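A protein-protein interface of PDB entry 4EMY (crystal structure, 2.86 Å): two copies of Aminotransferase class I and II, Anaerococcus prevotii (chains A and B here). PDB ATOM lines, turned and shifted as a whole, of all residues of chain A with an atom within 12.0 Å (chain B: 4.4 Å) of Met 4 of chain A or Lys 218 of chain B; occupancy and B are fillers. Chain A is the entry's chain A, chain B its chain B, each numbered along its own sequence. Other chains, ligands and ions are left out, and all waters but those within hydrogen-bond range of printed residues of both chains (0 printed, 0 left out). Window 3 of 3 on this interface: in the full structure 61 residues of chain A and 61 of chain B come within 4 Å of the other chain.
Of chain B, only Lys 218 comes within 4 Å of Met 4 of chain A.
Of the printed residues of chain B, Pro 5 of chain A touches Arg 179 and Lys 218.
Printed residues of chain B within 4 Å of Met 6 of chain A: Arg 179 (2.5 Å), Lys 218 (3.9 Å), Ile 219 (3.9 Å), Thr 220 (3.5 Å) and Asn 250 (3.97 Å).
Of the printed residues of chain B, Thr 7 of chain A touches Arg 179.
Printed residues of chain B within 4 Å of Ile 8 of chain A: Arg 179.
Of chain A, only Pro 5 (3.7 Å), Met 6 (2.5 Å), Thr 7 (3.6 Å) and Ile 8 (3.8 Å) come within 4 Å of Arg 179 of chain B.
Asp 216 of chain B touches none of the printed residues of chain A.
Printed residues of chain A within 4 Å of Lys 218 of chain B: Met 4, Pro 5 and Met 6.
Asn 250 of chain B touches just one residue of chain A: Met 6.
The nearest residue of chain A that does not touch Lys 218 of chain B is Thr 7 of chain A (5.9 Å).
No position is printed for both chains.
Among the printed residues, merely in contact across the chains: Pro 5 of chain A with Lys 218 of chain B (3.2 Å), Met 4 of chain A with Lys 218 of chain B (3.4 Å), Met 6 of chain A with Thr 220 of chain B (3.5 Å), Thr 7 of chain A with Arg 179 of chain B (3.6 Å), Pro 5 of chain A with Arg 179 of chain B (3.7 Å), Ile 8 of chain A with Arg 179 of chain B (3.8 Å), Met 6 of chain A with Lys 218 of chain B (3.9 Å), Met 6 of chain A with Ile 219 of chain B (3.9 Å) and Met 6 of chain A with Asn 250 of chain B (3.97 Å).
The backbone carbonyl oxygen (O) of Met 6 of chain A sits at hydrogen-bond distance from the guanidinium group (NH2) of Arg 179 of chain B (2.5 Å).
The side-chain hydroxyl (OG1) of Thr 12 of chain A sits at hydrogen-bond distance from the side-chain hydroxyl (OG1) of Thr 7 of chain A, 3.0 Å away.
The backbone carbonyl oxygen (O) of Ile 8 of chain A sits at hydrogen-bond distance from the side-chain hydroxyl (OG1) of Thr 12 of chain A, at 2.6 Å.
O of Asp 178 of chain B sits at hydrogen-bond distance from N of Lys 218 of chain B, at 2.8 Å.
The backbone NH (N) of Thr 220 of chain B is in hydrogen-bond range of the backbone carbonyl oxygen (O) of Ile 180 of chain B.
O of Lys 217 of chain B is in hydrogen-bond range of ND2 of Asn 250 of chain B, at 2.9 Å.
N of Ile 219 of chain B is in hydrogen-bond range of O of Asn 250 of chain B (2.8 Å).
Of the 9 printed residues of chain B, 5 touch a printed residue of chain A.
Printed residues of chain B that touch a printed residue of chain A: Arg 179, Lys 218, Ile 219, Thr 220 and Asn 250.
Hydrophobic or aromatic side chains of chain A that line the printed part of chain B: Met 4, Met 6 and Ile 8.
Among the printed residues, no Asp or Glu carboxylate lies within 4 Å of a Lys or Arg side-chain nitrogen of the other chain.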
ATOM      1  N   MET A   4      24.081 -14.362  31.422  1.00  0.00           N
ATOM      2  CA  MET A   4      23.828 -15.755  30.944  1.00  0.00           C
ATOM      3  C   MET A   4      25.015 -16.348  30.168  1.00  0.00           C
ATOM      4  O   MET A   4      25.433 -15.804  29.143  1.00  0.00           O
ATOM      5  CB  MET A   4      22.543 -15.820  30.109  1.00  0.00           C
ATOM      6  CG  MET A   4      21.266 -16.118  30.906  1.00  0.00           C
ATOM      7  SD  MET A   4      21.214 -17.926  31.688  1.00  0.00           S
ATOM      8  CE  MET A   4      21.739 -17.489  33.524  1.00  0.00           C
ATOM      9  N   PRO A   5      25.558 -17.473  30.661  1.00  0.00           N
ATOM     10  CA  PRO A   5      26.675 -18.141  30.003  1.00  0.00           C
ATOM     11  C   PRO A   5      26.235 -19.095  28.889  1.00  0.00           C
ATOM     12  O   PRO A   5      25.164 -19.696  28.973  1.00  0.00           O
ATOM     13  CB  PRO A   5      27.327 -18.920  31.144  1.00  0.00           C
ATOM     14  CG  PRO A   5      26.219 -19.205  32.099  1.00  0.00           C
ATOM     15  CD  PRO A   5      25.174 -18.141  31.919  1.00  0.00           C
ATOM     16  N   MET A   6      27.066 -19.228  27.857  1.00  0.00           N
ATOM     17  CA  MET A   6      26.811 -20.181  26.777  1.00  0.00           C
ATOM     18  C   MET A   6      27.095 -21.614  27.225  1.00  0.00           C
ATOM     19  O   MET A   6      26.439 -22.559  26.774  1.00  0.00           O
ATOM     20  CB  MET A   6      27.650 -19.848  25.538  1.00  0.00           C
ATOM     21  CG  MET A   6      26.962 -18.968  24.501  1.00  0.00           C
ATOM     22  SD  MET A   6      25.260 -19.641  23.811  1.00  0.00           S
ATOM     23  CE  MET A   6      25.796 -21.430  23.237  1.00  0.00           C
ATOM     24  N   THR A   7      28.080 -21.761  28.107  1.00  0.00           N
ATOM     25  CA  THR A   7      28.478 -23.060  28.637  1.00  0.00           C
ATOM     26  C   THR A   7      27.529 -23.492  29.751  1.00  0.00           C
ATOM     27  O   THR A   7      26.901 -22.652  30.393  1.00  0.00           O
ATOM     28  CB  THR A   7      29.913 -23.018  29.196  1.00  0.00           C
ATOM     29  OG1 THR A   7      30.050 -21.890  30.065  1.00  0.00           O
ATOM     30  CG2 THR A   7      30.929 -22.907  28.080  1.00  0.00           C
ATOM     31  N   ILE A   8      27.428 -24.803  29.967  1.00  0.00           N
ATOM     32  CA  ILE A   8      26.589 -25.362  31.031  1.00  0.00           C
ATOM     33  C   ILE A   8      27.225 -25.149  32.414  1.00  0.00           C
ATOM     34  O   ILE A   8      28.422 -24.877  32.511  1.00  0.00           O
ATOM     35  CB  ILE A   8      26.266 -26.857  30.785  1.00  0.00           C
ATOM     36  CG1 ILE A   8      27.534 -27.709  30.804  1.00  0.00           C
ATOM     37  CG2 ILE A   8      25.535 -27.035  29.462  1.00  0.00           C
ATOM     38  CD1 ILE A   8      27.283 -29.191  30.959  1.00  0.00           C
ATOM     39  N   LYS A   9      26.417 -25.265  33.469  1.00  0.00           N
ATOM     40  CA  LYS A   9      26.880 -25.079  34.858  1.00  0.00           C
ATOM     41  C   LYS A   9      28.175 -25.837  35.195  1.00  0.00           C
ATOM     42  O   LYS A   9      29.070 -25.293  35.845  1.00  0.00           O
ATOM     43  CB  LYS A   9      25.776 -25.466  35.857  1.00  0.00           C
ATOM     44  CG  LYS A   9      24.612 -24.491  35.950  1.00  0.00           C
ATOM     45  CD  LYS A   9      24.973 -23.266  36.780  1.00  0.00           C
ATOM     46  CE  LYS A   9      23.816 -22.278  36.864  1.00  0.00           C
ATOM     47  NZ  LYS A   9      24.169 -21.072  37.669  1.00  0.00           N
ATOM     48  N   ARG A  10      28.255 -27.090  34.751  1.00  0.00           N
ATOM     49  CA  ARG A  10      29.426 -27.944  34.965  1.00  0.00           C
ATOM     50  C   ARG A  10      30.637 -27.489  34.162  1.00  0.00           C
ATOM     51  O   ARG A  10      31.780 -27.650  34.597  1.00  0.00           O
ATOM     52  CB  ARG A  10      29.100 -29.390  34.583  1.00  0.00           C
ATOM     53  CG  ARG A  10      28.248 -30.132  35.592  1.00  0.00           C
ATOM     54  CD  ARG A  10      29.112 -30.808  36.644  1.00  0.00           C
ATOM     55  NE  ARG A  10      28.309 -31.672  37.503  1.00  0.00           N
ATOM     56  CZ  ARG A  10      27.972 -32.926  37.211  1.00  0.00           C
ATOM     57  NH1 ARG A  10      28.370 -33.486  36.073  1.00  0.00           N
ATOM     58  NH2 ARG A  10      27.237 -33.623  38.063  1.00  0.00           N
ATOM     59  N   ALA A  11      30.374 -26.933  32.984  1.00  0.00           N
ATOM     60  CA  ALA A  11      31.428 -26.529  32.061  1.00  0.00           C
ATOM     61  C   ALA A  11      31.863 -25.067  32.236  1.00  0.00           C
ATOM     62  O   ALA A  11      32.798 -24.618  31.575  1.00  0.00           O
ATOM     63  CB  ALA A  11      30.995 -26.799  30.628  1.00  0.00           C
ATOM     64  N   THR A  12      31.198 -24.334  33.127  1.00  0.00           N
ATOM     65  CA  THR A  12      31.565 -22.944  33.403  1.00  0.00           C
ATOM     66  C   THR A  12      32.588 -22.878  34.540  1.00  0.00           C
ATOM     67  O   THR A  12      32.377 -23.440  35.617  1.00  0.00           O
ATOM     68  CB  THR A  12      30.334 -22.069  33.725  1.00  0.00           C
ATOM     69  OG1 THR A  12      29.241 -22.426  32.866  1.00  0.00           O
ATOM     70  CG2 THR A  12      30.663 -20.595  33.526  1.00  0.00           C
ATOM     71  N   TRP A  13      33.702 -22.199  34.283  1.00  0.00           N
ATOM     72  CA  TRP A  13      34.808 -22.142  35.232  1.00  0.00           C
ATOM     73  C   TRP A  13      35.226 -20.733  35.522  1.00  0.00           C
ATOM     74  O   TRP A  13      36.070 -20.159  34.825  1.00  0.00           O
ATOM     75  CB  TRP A  13      35.987 -22.971  34.730  1.00  0.00           C
ATOM     76  CG  TRP A  13      35.627 -24.422  34.545  1.00  0.00           C
ATOM     77  CD1 TRP A  13      35.448 -25.108  33.347  1.00  0.00           C
ATOM     78  CD2 TRP A  13      35.352 -25.414  35.597  1.00  0.00           C
ATOM     79  NE1 TRP A  13      35.106 -26.420  33.577  1.00  0.00           N
ATOM     80  CE2 TRP A  13      35.030 -26.668  34.904  1.00  0.00           C
ATOM     81  CE3 TRP A  13      35.346 -25.392  36.989  1.00  0.00           C
ATOM     82  CZ2 TRP A  13      34.720 -27.829  35.594  1.00  0.00           C
ATOM     83  CZ3 TRP A  13      35.031 -26.570  37.672  1.00  0.00           C
ATOM     84  CH2 TRP A  13      34.728 -27.758  36.990  1.00  0.00           C
ATOM     85  N   ASN A  14      34.629 -20.163  36.566  1.00  0.00           N
ATOM     86  CA  ASN A  14      35.010 -18.843  37.068  1.00  0.00           C
ATOM     87  C   ASN A  14      36.366 -18.943  37.781  1.00  0.00           C
ATOM     88  O   ASN A  14      36.563 -18.378  38.860  1.00  0.00           O
ATOM     89  CB  ASN A  14      33.932 -18.287  38.018  1.00  0.00           C
ATOM     90  CG  ASN A  14      32.510 -18.498  37.500  1.00  0.00           C
ATOM     91  OD1 ASN A  14      32.054 -17.807  36.586  1.00  0.00           O
ATOM     92  ND2 ASN A  14      31.798 -19.448  38.101  1.00  0.00           N
ATOM     93  N   ASP B 178      15.667 -25.337  26.215  1.00  0.00           N
ATOM     94  CA  ASP B 178      16.116 -23.969  26.062  1.00  0.00           C
ATOM     95  C   ASP B 178      17.549 -23.977  25.544  1.00  0.00           C
ATOM     96  O   ASP B 178      18.137 -22.926  25.281  1.00  0.00           O
ATOM     97  CB  ASP B 178      15.991 -23.206  27.388  1.00  0.00           C
ATOM     98  CG  ASP B 178      14.543 -22.828  27.722  1.00  0.00           C
ATOM     99  OD1 ASP B 178      13.732 -22.618  26.789  1.00  0.00           O
ATOM    100  OD2 ASP B 178      14.210 -22.731  28.923  1.00  0.00           O
ATOM    101  N   ARG B 179      18.104 -25.174  25.385  1.00  0.00           N
ATOM    102  CA  ARG B 179      19.452 -25.331  24.854  1.00  0.00           C
ATOM    103  C   ARG B 179      19.520 -26.538  23.917  1.00  0.00           C
ATOM    104  O   ARG B 179      19.118 -27.645  24.287  1.00  0.00           O
ATOM    105  CB  ARG B 179      20.471 -25.434  25.997  1.00  0.00           C
ATOM    106  CG  ARG B 179      21.775 -26.122  25.639  1.00  0.00           C
ATOM    107  CD  ARG B 179      22.705 -26.230  26.835  1.00  0.00           C
ATOM    108  NE  ARG B 179      23.559 -25.054  26.956  1.00  0.00           N
ATOM    109  CZ  ARG B 179      23.472 -24.159  27.933  1.00  0.00           C
ATOM    110  NH1 ARG B 179      22.573 -24.292  28.899  1.00  0.00           N
ATOM    111  NH2 ARG B 179      24.291 -23.125  27.948  1.00  0.00           N
ATOM    112  N   ILE B 180      20.009 -26.301  22.701  1.00  0.00           N
ATOM    113  CA  ILE B 180      20.141 -27.341  21.675  1.00  0.00           C
ATOM    114  C   ILE B 180      21.466 -27.218  20.915  1.00  0.00           C
ATOM    115  O   ILE B 180      22.168 -26.201  21.016  1.00  0.00           O
ATOM    116  CB  ILE B 180      18.980 -27.309  20.646  1.00  0.00           C
ATOM    117  CG1 ILE B 180      19.044 -26.030  19.796  1.00  0.00           C
ATOM    118  CG2 ILE B 180      17.629 -27.470  21.336  1.00  0.00           C
ATOM    119  CD1 ILE B 180      18.585 -26.205  18.363  1.00  0.00           C
ATOM    120  N   ASP B 216      15.870 -16.628  25.206  1.00  0.00           N
ATOM    121  CA  ASP B 216      15.890 -17.678  26.230  1.00  0.00           C
ATOM    122  C   ASP B 216      16.539 -18.941  25.672  1.00  0.00           C
ATOM    123  O   ASP B 216      16.958 -19.821  26.425  1.00  0.00           O
ATOM    124  CB  ASP B 216      14.475 -18.011  26.712  1.00  0.00           C
ATOM    125  CG  ASP B 216      13.846 -16.891  27.516  1.00  0.00           C
ATOM    126  OD1 ASP B 216      14.564 -16.227  28.295  1.00  0.00           O
ATOM    127  OD2 ASP B 216      12.621 -16.683  27.376  1.00  0.00           O
ATOM    128  N   LYS B 217      16.607 -19.019  24.346  1.00  0.00           N
ATOM    129  CA  LYS B 217      17.201 -20.159  23.658  1.00  0.00           C
ATOM    130  C   LYS B 217      18.700 -19.965  23.446  1.00  0.00           C
ATOM    131  O   LYS B 217      19.154 -18.876  23.098  1.00  0.00           O
ATOM    132  CB  LYS B 217      16.510 -20.399  22.308  1.00  0.00           C
ATOM    133  CG  LYS B 217      15.003 -20.597  22.375  1.00  0.00           C
ATOM    134  CD  LYS B 217      14.618 -21.862  23.130  1.00  0.00           C
ATOM    135  CE  LYS B 217      13.137 -21.867  23.474  1.00  0.00           C
ATOM    136  NZ  LYS B 217      12.755 -23.045  24.296  1.00  0.00           N
ATOM    137  N   LYS B 218      19.464 -21.025  23.668  1.00  0.00           N
ATOM    138  CA  LYS B 218      20.878 -21.018  23.324  1.00  0.00           C
ATOM    139  C   LYS B 218      21.156 -22.132  22.325  1.00  0.00           C
ATOM    140  O   LYS B 218      20.753 -23.275  22.532  1.00  0.00           O
ATOM    141  CB  LYS B 218      21.748 -21.146  24.577  1.00  0.00           C
ATOM    142  CG  LYS B 218      21.660 -19.931  25.487  1.00  0.00           C
ATOM    143  CD  LYS B 218      22.616 -20.034  26.659  1.00  0.00           C
ATOM    144  CE  LYS B 218      22.319 -18.958  27.697  1.00  0.00           C
ATOM    145  NZ  LYS B 218      22.685 -17.588  27.236  1.00  0.00           N
ATOM    146  N   ILE B 219      21.817 -21.785  21.224  1.00  0.00           N
ATOM    147  CA  ILE B 219      22.030 -22.720  20.122  1.00  0.00           C
ATOM    148  C   ILE B 219      23.513 -22.848  19.791  1.00  0.00           C
ATOM    149  O   ILE B 219      24.214 -21.844  19.663  1.00  0.00           O
ATOM    150  CB  ILE B 219      21.263 -22.282  18.856  1.00  0.00           C
ATOM    151  CG1 ILE B 219      19.813 -21.925  19.196  1.00  0.00           C
ATOM    152  CG2 ILE B 219      21.298 -23.378  17.796  1.00  0.00           C
ATOM    153  CD1 ILE B 219      19.118 -21.095  18.141  1.00  0.00           C
ATOM    154  N   THR B 220      23.988 -24.085  19.660  1.00  0.00           N
ATOM    155  CA  THR B 220      25.378 -24.331  19.291  1.00  0.00           C
ATOM    156  C   THR B 220      25.469 -25.128  18.001  1.00  0.00           C
ATOM    157  O   THR B 220      24.949 -26.240  17.907  1.00  0.00           O
ATOM    158  CB  THR B 220      26.144 -25.066  20.396  1.00  0.00           C
ATOM    159  OG1 THR B 220      25.794 -24.507  21.670  1.00  0.00           O
ATOM    160  CG2 THR B 220      27.643 -24.931  20.171  1.00  0.00           C
ATOM    161  N   ASN B 250      23.687 -15.692  21.344  1.00  0.00           N
ATOM    162  CA  ASN B 250      23.176 -17.023  21.677  1.00  0.00           C
ATOM    163  C   ASN B 250      23.297 -18.059  20.546  1.00  0.00           C
ATOM    164  O   ASN B 250      22.785 -19.178  20.673  1.00  0.00           O
ATOM    165  CB  ASN B 250      21.743 -16.951  22.231  1.00  0.00           C
ATOM    166  CG  ASN B 250      20.783 -16.216  21.311  1.00  0.00           C
ATOM    167  OD1 ASN B 250      21.183 -15.363  20.521  1.00  0.00           O
ATOM    168  ND2 ASN B 250      19.499 -16.538  21.423  1.00  0.00           N
